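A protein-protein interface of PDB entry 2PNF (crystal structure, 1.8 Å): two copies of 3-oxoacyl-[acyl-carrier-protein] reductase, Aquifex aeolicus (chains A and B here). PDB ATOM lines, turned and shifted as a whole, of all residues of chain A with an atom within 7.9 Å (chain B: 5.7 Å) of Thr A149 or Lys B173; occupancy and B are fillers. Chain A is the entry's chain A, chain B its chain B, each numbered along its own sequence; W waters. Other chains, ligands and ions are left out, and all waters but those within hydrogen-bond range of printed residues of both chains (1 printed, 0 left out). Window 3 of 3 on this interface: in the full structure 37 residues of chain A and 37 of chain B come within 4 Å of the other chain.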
ATOM      1  N   SER A 144      29.857 -22.517 -36.675  1.00  0.00           N
ATOM      2  CA  SER A 144      28.502 -22.162 -36.171  1.00  0.00           C
ATOM      3  C   SER A 144      28.506 -20.774 -35.591  1.00  0.00           C
ATOM      4  O   SER A 144      29.498 -20.328 -35.018  1.00  0.00           O
ATOM      5  CB  SER A 144      28.047 -23.147 -35.053  1.00  0.00           C
ATOM      6  OG  SER A 144      26.881 -22.695 -34.347  1.00  0.00           O
ATOM      7  N   VAL A 145      27.383 -20.081 -35.730  1.00  0.00           N
ATOM      8  CA  VAL A 145      27.263 -18.769 -35.170  1.00  0.00           C
ATOM      9  C   VAL A 145      27.628 -18.826 -33.678  1.00  0.00           C
ATOM     10  O   VAL A 145      28.137 -17.849 -33.122  1.00  0.00           O
ATOM     11  CB  VAL A 145      25.764 -18.241 -35.308  1.00  0.00           C
ATOM     12  CG1 VAL A 145      24.794 -19.134 -34.487  1.00  0.00           C
ATOM     13  CG2 VAL A 145      25.669 -16.816 -34.825  1.00  0.00           C
ATOM     14  N   VAL A 146      27.384 -19.968 -33.034  1.00  0.00           N
ATOM     15  CA  VAL A 146      27.645 -20.110 -31.597  1.00  0.00           C
ATOM     16  C   VAL A 146      29.154 -20.065 -31.227  1.00  0.00           C
ATOM     17  O   VAL A 146      29.527 -19.741 -30.082  1.00  0.00           O
ATOM     18  CB  VAL A 146      26.877 -21.382 -31.094  1.00  0.00           C
ATOM     19  CG1 VAL A 146      27.499 -21.983 -29.928  1.00  0.00           C
ATOM     20  CG2 VAL A 146      25.424 -20.962 -30.794  1.00  0.00           C
ATOM     21  N   GLY A 147      30.010 -20.326 -32.211  1.00  0.00           N
ATOM     22  CA  GLY A 147      31.452 -20.245 -31.974  1.00  0.00           C
ATOM     23  C   GLY A 147      31.852 -18.784 -31.893  1.00  0.00           C
ATOM     24  O   GLY A 147      32.933 -18.446 -31.399  1.00  0.00           O
ATOM     25  N   PHE A 148      30.970 -17.891 -32.360  1.00  0.00           N
ATOM     26  CA  PHE A 148      31.274 -16.454 -32.334  1.00  0.00           C
ATOM     27  C   PHE A 148      30.609 -15.681 -31.206  1.00  0.00           C
ATOM     28  O   PHE A 148      31.188 -14.743 -30.640  1.00  0.00           O
ATOM     29  CB  PHE A 148      30.856 -15.821 -33.665  1.00  0.00           C
ATOM     30  CG  PHE A 148      31.686 -16.279 -34.810  1.00  0.00           C
ATOM     31  CD1 PHE A 148      32.780 -15.529 -35.245  1.00  0.00           C
ATOM     32  CD2 PHE A 148      31.435 -17.519 -35.393  1.00  0.00           C
ATOM     33  CE1 PHE A 148      33.623 -16.019 -36.258  1.00  0.00           C
ATOM     34  CE2 PHE A 148      32.264 -18.018 -36.392  1.00  0.00           C
ATOM     35  CZ  PHE A 148      33.364 -17.251 -36.818  1.00  0.00           C
ATOM     36  N   THR A 149      29.372 -16.072 -30.907  1.00  0.00           N
ATOM     37  CA  THR A 149      28.599 -15.436 -29.875  1.00  0.00           C
ATOM     38  C   THR A 149      28.702 -16.132 -28.526  1.00  0.00           C
ATOM     39  O   THR A 149      28.502 -15.493 -27.484  1.00  0.00           O
ATOM     40  CB  THR A 149      27.102 -15.424 -30.264  1.00  0.00           C
ATOM     41  OG1 THR A 149      26.601 -16.763 -30.280  1.00  0.00           O
ATOM     42  CG2 THR A 149      26.915 -14.827 -31.648  1.00  0.00           C
ATOM     43  N   GLY A 150      29.038 -17.422 -28.532  1.00  0.00           N
ATOM     44  CA  GLY A 150      29.032 -18.186 -27.289  1.00  0.00           C
ATOM     45  C   GLY A 150      27.565 -18.600 -27.075  1.00  0.00           C
ATOM     46  O   GLY A 150      26.669 -17.994 -27.682  1.00  0.00           O
ATOM     47  N   ASN A 151      27.302 -19.618 -26.245  1.00  0.00           N
ATOM     48  CA  ASN A 151      25.910 -20.050 -25.991  1.00  0.00           C
ATOM     49  C   ASN A 151      25.857 -20.807 -24.687  1.00  0.00           C
ATOM     50  O   ASN A 151      26.667 -21.709 -24.452  1.00  0.00           O
ATOM     51  CB  ASN A 151      25.394 -20.986 -27.121  1.00  0.00           C
ATOM     52  CG  ASN A 151      23.872 -21.233 -27.042  1.00  0.00           C
ATOM     53  OD1 ASN A 151      23.122 -20.354 -26.648  1.00  0.00           O
ATOM     54  ND2 ASN A 151      23.430 -22.422 -27.437  1.00  0.00           N
ATOM     55  N   VAL A 152      24.899 -20.453 -23.841  1.00  0.00           N
ATOM     56  CA  VAL A 152      24.686 -21.135 -22.559  1.00  0.00           C
ATOM     57  C   VAL A 152      24.449 -22.632 -22.790  1.00  0.00           C
ATOM     58  O   VAL A 152      23.695 -23.025 -23.696  1.00  0.00           O
ATOM     59  CB  VAL A 152      23.453 -20.507 -21.828  1.00  0.00           C
ATOM     60  CG1 VAL A 152      22.995 -21.404 -20.671  1.00  0.00           C
ATOM     61  CG2 VAL A 152      23.814 -19.141 -21.279  1.00  0.00           C
ATOM     62  N   GLY A 153      25.121 -23.465 -21.987  1.00  0.00           N
ATOM     63  CA  GLY A 153      24.992 -24.905 -22.069  1.00  0.00           C
ATOM     64  C   GLY A 153      25.833 -25.535 -23.158  1.00  0.00           C
ATOM     65  O   GLY A 153      25.790 -26.753 -23.347  1.00  0.00           O
ATOM     66  N   VAL A 155      29.406 -24.623 -23.735  1.00  0.00           N
ATOM     67  CA  VAL A 155      30.773 -24.131 -23.678  1.00  0.00           C
ATOM     68  C   VAL A 155      31.716 -25.067 -24.510  1.00  0.00           C
ATOM     69  O   VAL A 155      32.652 -24.562 -25.161  1.00  0.00           O
ATOM     70  CB  VAL A 155      31.280 -24.015 -22.244  1.00  0.00           C
ATOM     71  CG1 VAL A 155      32.784 -23.641 -22.252  1.00  0.00           C
ATOM     72  CG2 VAL A 155      30.464 -22.929 -21.496  1.00  0.00           C
ATOM     73  N   SER A 158      30.842 -24.501 -28.364  1.00  0.00           N
ATOM     74  CA  SER A 158      31.303 -23.175 -28.784  1.00  0.00           C
ATOM     75  C   SER A 158      32.835 -23.092 -28.891  1.00  0.00           C
ATOM     76  O   SER A 158      33.365 -22.446 -29.801  1.00  0.00           O
ATOM     77  CB  SER A 158      30.811 -22.106 -27.821  1.00  0.00           C
ATOM     78  OG  SER A 158      31.266 -20.855 -28.270  1.00  0.00           O
ATOM     79  N   ALA A 162      34.654 -22.145 -32.422  1.00  0.00           N
ATOM     80  CA  ALA A 162      35.553 -21.007 -32.496  1.00  0.00           C
ATOM     81  C   ALA A 162      36.960 -21.564 -32.853  1.00  0.00           C
ATOM     82  O   ALA A 162      37.705 -20.952 -33.608  1.00  0.00           O
ATOM     83  CB  ALA A 162      35.637 -20.304 -31.157  1.00  0.00           C
ATOM     84  N   PHE A 189      20.669 -20.450 -37.345  1.00  0.00           N
ATOM     85  CA  PHE A 189      19.602 -21.412 -36.969  1.00  0.00           C
ATOM     86  C   PHE A 189      19.001 -21.995 -38.237  1.00  0.00           C
ATOM     87  O   PHE A 189      18.335 -21.312 -38.991  1.00  0.00           O
ATOM     88  CB  PHE A 189      18.530 -20.697 -36.134  1.00  0.00           C
ATOM     89  CG  PHE A 189      19.059 -20.164 -34.828  1.00  0.00           C
ATOM     90  CD1 PHE A 189      20.215 -20.715 -34.264  1.00  0.00           C
ATOM     91  CD2 PHE A 189      18.430 -19.111 -34.175  1.00  0.00           C
ATOM     92  CE1 PHE A 189      20.741 -20.223 -33.063  1.00  0.00           C
ATOM     93  CE2 PHE A 189      18.942 -18.609 -32.967  1.00  0.00           C
ATOM     94  CZ  PHE A 189      20.101 -19.164 -32.410  1.00  0.00           C
ATOM     95  N   GLN A 209      15.290 -13.800 -32.865  1.00  0.00           N
ATOM     96  CA  GLN A 209      16.688 -13.375 -32.924  1.00  0.00           C
ATOM     97  C   GLN A 209      17.137 -13.226 -34.367  1.00  0.00           C
ATOM     98  O   GLN A 209      18.258 -12.778 -34.610  1.00  0.00           O
ATOM     99  CB  GLN A 209      17.624 -14.410 -32.287  1.00  0.00           C
ATOM    100  CG  GLN A 209      17.541 -14.578 -30.767  1.00  0.00           C
ATOM    101  CD  GLN A 209      18.528 -15.629 -30.269  1.00  0.00           C
ATOM    102  OE1 GLN A 209      19.726 -15.361 -30.091  1.00  0.00           O
ATOM    103  NE2 GLN A 209      18.039 -16.832 -30.067  1.00  0.00           N
ATOM    104  N   HIS A 242      29.311 -16.227 -42.837  1.00  0.00           N
ATOM    105  CA  HIS A 242      28.198 -16.457 -41.917  1.00  0.00           C
ATOM    106  C   HIS A 242      26.939 -16.572 -42.728  1.00  0.00           C
ATOM    107  O   HIS A 242      26.694 -15.733 -43.592  1.00  0.00           O
ATOM    108  CB  HIS A 242      28.099 -15.264 -40.964  1.00  0.00           C
ATOM    109  CG  HIS A 242      29.305 -15.116 -40.096  1.00  0.00           C
ATOM    110  ND1 HIS A 242      29.373 -15.685 -38.850  1.00  0.00           N
ATOM    111  CD2 HIS A 242      30.485 -14.467 -40.287  1.00  0.00           C
ATOM    112  CE1 HIS A 242      30.539 -15.392 -38.296  1.00  0.00           C
ATOM    113  NE2 HIS A 242      31.233 -14.655 -39.152  1.00  0.00           N
ATOM    114  N   ASN A 244      23.366 -16.802 -41.596  1.00  0.00           N
ATOM    115  CA  ASN A 244      22.490 -16.814 -40.435  1.00  0.00           C
ATOM    116  C   ASN A 244      21.325 -15.867 -40.465  1.00  0.00           C
ATOM    117  O   ASN A 244      20.813 -15.508 -39.410  1.00  0.00           O
ATOM    118  CB  ASN A 244      23.331 -16.490 -39.191  1.00  0.00           C
ATOM    119  CG  ASN A 244      23.994 -15.113 -39.275  1.00  0.00           C
ATOM    120  OD1 ASN A 244      23.399 -14.153 -39.772  1.00  0.00           O
ATOM    121  ND2 ASN A 244      25.229 -15.008 -38.774  1.00  0.00           N
ATOM    122  N   MET A 247      21.512 -12.556 -38.144  1.00  0.00           N
ATOM    123  CA  MET A 247      21.652 -12.679 -36.696  1.00  0.00           C
ATOM    124  C   MET A 247      22.976 -12.206 -36.119  1.00  0.00           C
ATOM    125  O   MET A 247      23.028 -11.742 -34.972  1.00  0.00           O
ATOM    126  CB  MET A 247      21.439 -14.130 -36.319  1.00  0.00           C
ATOM    127  CG  MET A 247      21.002 -14.306 -34.901  1.00  0.00           C
ATOM    128  SD  MET A 247      20.293 -15.958 -34.775  1.00  0.00           S
ATOM    129  CE  MET A 247      21.655 -16.855 -35.251  1.00  0.00           C
ATOM    130  N   PHE A 248      24.044 -12.307 -36.903  1.00  0.00           N
ATOM    131  CA  PHE A 248      25.356 -11.912 -36.411  1.00  0.00           C
ATOM    132  C   PHE A 248      26.179 -11.429 -37.601  1.00  0.00           C
ATOM    133  O   PHE A 248      26.254 -12.161 -38.622  1.00  0.00           O
ATOM    134  CB  PHE A 248      26.021 -13.125 -35.703  1.00  0.00           C
ATOM    135  CG  PHE A 248      27.445 -12.873 -35.238  1.00  0.00           C
ATOM    136  CD1 PHE A 248      27.694 -12.247 -34.025  1.00  0.00           C
ATOM    137  CD2 PHE A 248      28.525 -13.204 -36.052  1.00  0.00           C
ATOM    138  CE1 PHE A 248      29.014 -11.938 -33.624  1.00  0.00           C
ATOM    139  CE2 PHE A 248      29.830 -12.910 -35.680  1.00  0.00           C
ATOM    140  CZ  PHE A 248      30.085 -12.265 -34.454  1.00  0.00           C
ATOM    141  OXT PHE A 248      26.715 -10.301 -37.495  1.00  0.00           O
ATOM    142  N   THR B 168      35.557 -18.538 -23.595  1.00  0.00           N
ATOM    143  CA  THR B 168      35.401 -17.306 -22.827  1.00  0.00           C
ATOM    144  C   THR B 168      34.013 -16.727 -23.033  1.00  0.00           C
ATOM    145  O   THR B 168      33.318 -16.421 -22.077  1.00  0.00           O
ATOM    146  CB  THR B 168      36.434 -16.248 -23.314  1.00  0.00           C
ATOM    147  OG1 THR B 168      37.751 -16.727 -23.024  1.00  0.00           O
ATOM    148  CG2 THR B 168      36.235 -14.863 -22.632  1.00  0.00           C
ATOM    149  N   LYS B 169      33.594 -16.639 -24.284  1.00  0.00           N
ATOM    150  CA  LYS B 169      32.281 -16.014 -24.554  1.00  0.00           C
ATOM    151  C   LYS B 169      31.110 -16.808 -24.012  1.00  0.00           C
ATOM    152  O   LYS B 169      30.159 -16.215 -23.449  1.00  0.00           O
ATOM    153  CB  LYS B 169      32.133 -15.713 -26.046  1.00  0.00           C
ATOM    154  CG  LYS B 169      33.057 -14.510 -26.444  1.00  0.00           C
ATOM    155  CD  LYS B 169      32.881 -14.076 -27.870  1.00  0.00           C
ATOM    156  CE  LYS B 169      33.760 -12.864 -28.233  1.00  0.00           C
ATOM    157  NZ  LYS B 169      33.405 -11.594 -27.496  1.00  0.00           N
ATOM    158  N   SER B 170      31.180 -18.138 -24.147  1.00  0.00           N
ATOM    159  CA  SER B 170      30.115 -19.017 -23.632  1.00  0.00           C
ATOM    160  C   SER B 170      30.088 -19.059 -22.130  1.00  0.00           C
ATOM    161  O   SER B 170      29.011 -19.010 -21.506  1.00  0.00           O
ATOM    162  CB  SER B 170      30.282 -20.445 -24.140  1.00  0.00           C
ATOM    163  OG  SER B 170      30.017 -20.459 -25.510  1.00  0.00           O
ATOM    164  N   LEU B 171      31.265 -19.159 -21.525  1.00  0.00           N
ATOM    165  CA  LEU B 171      31.293 -19.242 -20.067  1.00  0.00           C
ATOM    166  C   LEU B 171      30.842 -17.903 -19.452  1.00  0.00           C
ATOM    167  O   LEU B 171      30.156 -17.873 -18.409  1.00  0.00           O
ATOM    168  CB  LEU B 171      32.698 -19.635 -19.570  1.00  0.00           C
ATOM    169  CG  LEU B 171      32.763 -19.997 -18.074  1.00  0.00           C
ATOM    170  CD1 LEU B 171      31.837 -21.188 -17.758  1.00  0.00           C
ATOM    171  CD2 LEU B 171      34.209 -20.354 -17.699  1.00  0.00           C
ATOM    172  N   ALA B 172      31.204 -16.802 -20.108  1.00  0.00           N
ATOM    173  CA  ALA B 172      30.818 -15.481 -19.642  1.00  0.00           C
ATOM    174  C   ALA B 172      29.271 -15.414 -19.580  1.00  0.00           C
ATOM    175  O   ALA B 172      28.705 -14.932 -18.599  1.00  0.00           O
ATOM    176  CB  ALA B 172      31.358 -14.445 -20.572  1.00  0.00           C
ATOM    177  N   LYS B 173      28.602 -15.891 -20.620  1.00  0.00           N
ATOM    178  CA  LYS B 173      27.140 -15.894 -20.617  1.00  0.00           C
ATOM    179  C   LYS B 173      26.547 -16.735 -19.491  1.00  0.00           C
ATOM    180  O   LYS B 173      25.591 -16.318 -18.837  1.00  0.00           O
ATOM    181  CB  LYS B 173      26.613 -16.370 -21.978  1.00  0.00           C
ATOM    182  CG  LYS B 173      26.878 -15.364 -23.068  1.00  0.00           C
ATOM    183  CD  LYS B 173      26.209 -15.708 -24.384  1.00  0.00           C
ATOM    184  CE  LYS B 173      26.464 -14.605 -25.392  1.00  0.00           C
ATOM    185  NZ  LYS B 173      25.737 -14.927 -26.642  1.00  0.00           N
ATOM    186  N   GLU B 174      27.082 -17.931 -19.253  1.00  0.00           N
ATOM    187  CA  GLU B 174      26.559 -18.772 -18.174  1.00  0.00           C
ATOM    188  C   GLU B 174      26.804 -18.237 -16.777  1.00  0.00           C
ATOM    189  O   GLU B 174      25.975 -18.419 -15.881  1.00  0.00           O
ATOM    190  CB  GLU B 174      27.145 -20.162 -18.236  1.00  0.00           C
ATOM    191  CG  GLU B 174      26.590 -20.999 -19.327  1.00  0.00           C
ATOM    192  CD  GLU B 174      27.107 -22.439 -19.260  1.00  0.00           C
ATOM    193  OE1 GLU B 174      27.413 -22.911 -18.129  1.00  0.00           O
ATOM    194  OE2 GLU B 174      27.182 -23.102 -20.333  1.00  0.00           O
ATOM    195  N   LEU B 175      27.910 -17.533 -16.578  1.00  0.00           N
ATOM    196  CA  LEU B 175      28.185 -17.080 -15.236  1.00  0.00           C
ATOM    197  C   LEU B 175      27.802 -15.643 -14.937  1.00  0.00           C
ATOM    198  O   LEU B 175      27.900 -15.211 -13.798  1.00  0.00           O
ATOM    199  CB  LEU B 175      29.681 -17.262 -14.909  1.00  0.00           C
ATOM    200  CG  LEU B 175      30.222 -18.690 -15.120  1.00  0.00           C
ATOM    201  CD1 LEU B 175      31.721 -18.746 -14.781  1.00  0.00           C
ATOM    202  CD2 LEU B 175      29.431 -19.683 -14.240  1.00  0.00           C
ATOM    203  N   ALA B 176      27.409 -14.904 -15.961  1.00  0.00           N
ATOM    204  CA  ALA B 176      27.099 -13.491 -15.802  1.00  0.00           C
ATOM    205  C   ALA B 176      26.039 -13.239 -14.732  1.00  0.00           C
ATOM    206  O   ALA B 176      26.156 -12.278 -13.962  1.00  0.00           O
ATOM    207  CB  ALA B 176      26.660 -12.912 -17.138  1.00  0.00           C
ATOM    208  N   PRO B 177      25.012 -14.103 -14.654  1.00  0.00           N
ATOM    209  CA  PRO B 177      23.979 -13.885 -13.628  1.00  0.00           C
ATOM    210  C   PRO B 177      24.543 -13.942 -12.213  1.00  0.00           C
ATOM    211  O   PRO B 177      23.937 -13.441 -11.265  1.00  0.00           O
ATOM    212  CB  PRO B 177      22.982 -15.021 -13.891  1.00  0.00           C
ATOM    213  CG  PRO B 177      23.079 -15.196 -15.363  1.00  0.00           C
ATOM    214  CD  PRO B 177      24.580 -15.138 -15.609  1.00  0.00           C
HETATM  215  O   HOH W   1      28.355 -25.174 -20.989  1.00  0.00           O
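O of Thr A149 is in hydrogen-bond range of NZ of Lys B173. O of Gly A150 is in hydrogen-bond range of NZ of Lys B173 (3.4 Å). The backbone NH (N) of Asn A151 is in hydrogen-bond range of the side-chain hydroxyl (OG) of Ser B170, at 2.9 Å. The side-chain carboxylate of Glu B174 is in hydrogen-bond range of the backbone NH of Gly A153. The side-chain hydroxyl (OG) of Ser B170 lies close to the side-chain hydroxyl (OG) of Ser A158 (3.1 Å).
The backbone carbonyl oxygen (O) of Val A145 lies within hydrogen-bond range of the side-chain hydroxyl (OG1) of Thr A149. The backbone carbonyl oxygen (O) of Val A146 sits at hydrogen-bond distance from the side-chain hydroxyl (OG) of Ser A158 (2.7 Å).
Among the printed residues, merely in contact across the chains: Phe A148 with Lys B169 (3.3 Å), Thr A149 with Lys B169 (3.9 Å), Gly A150 with Ser B170 (3.0 Å), Val A152 with Glu B174 (3.7 Å), Val A155 with Ser B170 (3.6 Å), Val A155 with Leu B171 (3.9 Å) and Val A155 with Glu B174 (3.5 Å).
Of the printed residues of chain B, Gly A150 touches Ser B170 (3.0 Å) and Lys B173 (3.4 Å). Of the printed residues of chain B, Asn A151 touches Ser B170. Of the printed residues of chain B, Gly A153 touches Glu B174 (2.7 Å). Of the printed residues of chain B, Val A155 touches Ser B170 (3.6 Å), Leu B171 (3.9 Å) and Glu B174 (3.5 Å). Printed residues of chain B within 4 Å of Ser A158: Ser B170 (2.9 Å). No residue of chain A comes within 4 Å of Ala B172. Of the printed residues of chain A, Lys B173 touches Thr A149 and Gly A150.
Of the 10 printed residues of chain B, 5 touch a printed residue of chain A. Printed residues of chain B that touch a printed residue of chain A: Lys B169, Ser B170, Leu B171, Lys B173 and Glu B174. Of the 19 printed residues of chain A, 8 touch a printed residue of chain B. Hydrophobic or aromatic side chains of chain A that line the printed part of chain B: Val A152 and Val A155. Among the printed residues, 12 pairs touch across the chains. Among the printed residues, no Asp or Glu carboxylate lies within 4 Å of a Lys or Arg side-chain nitrogen of the other chain.
No position is printed for both chains. Of the 12 pairs that touch across the chains among the printed residues, none has its exchanged pair printed and touching as well.
Water W1 bridges OE2 of Glu B174 (2.5 Å) and N of Val A155 (3.0 Å).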
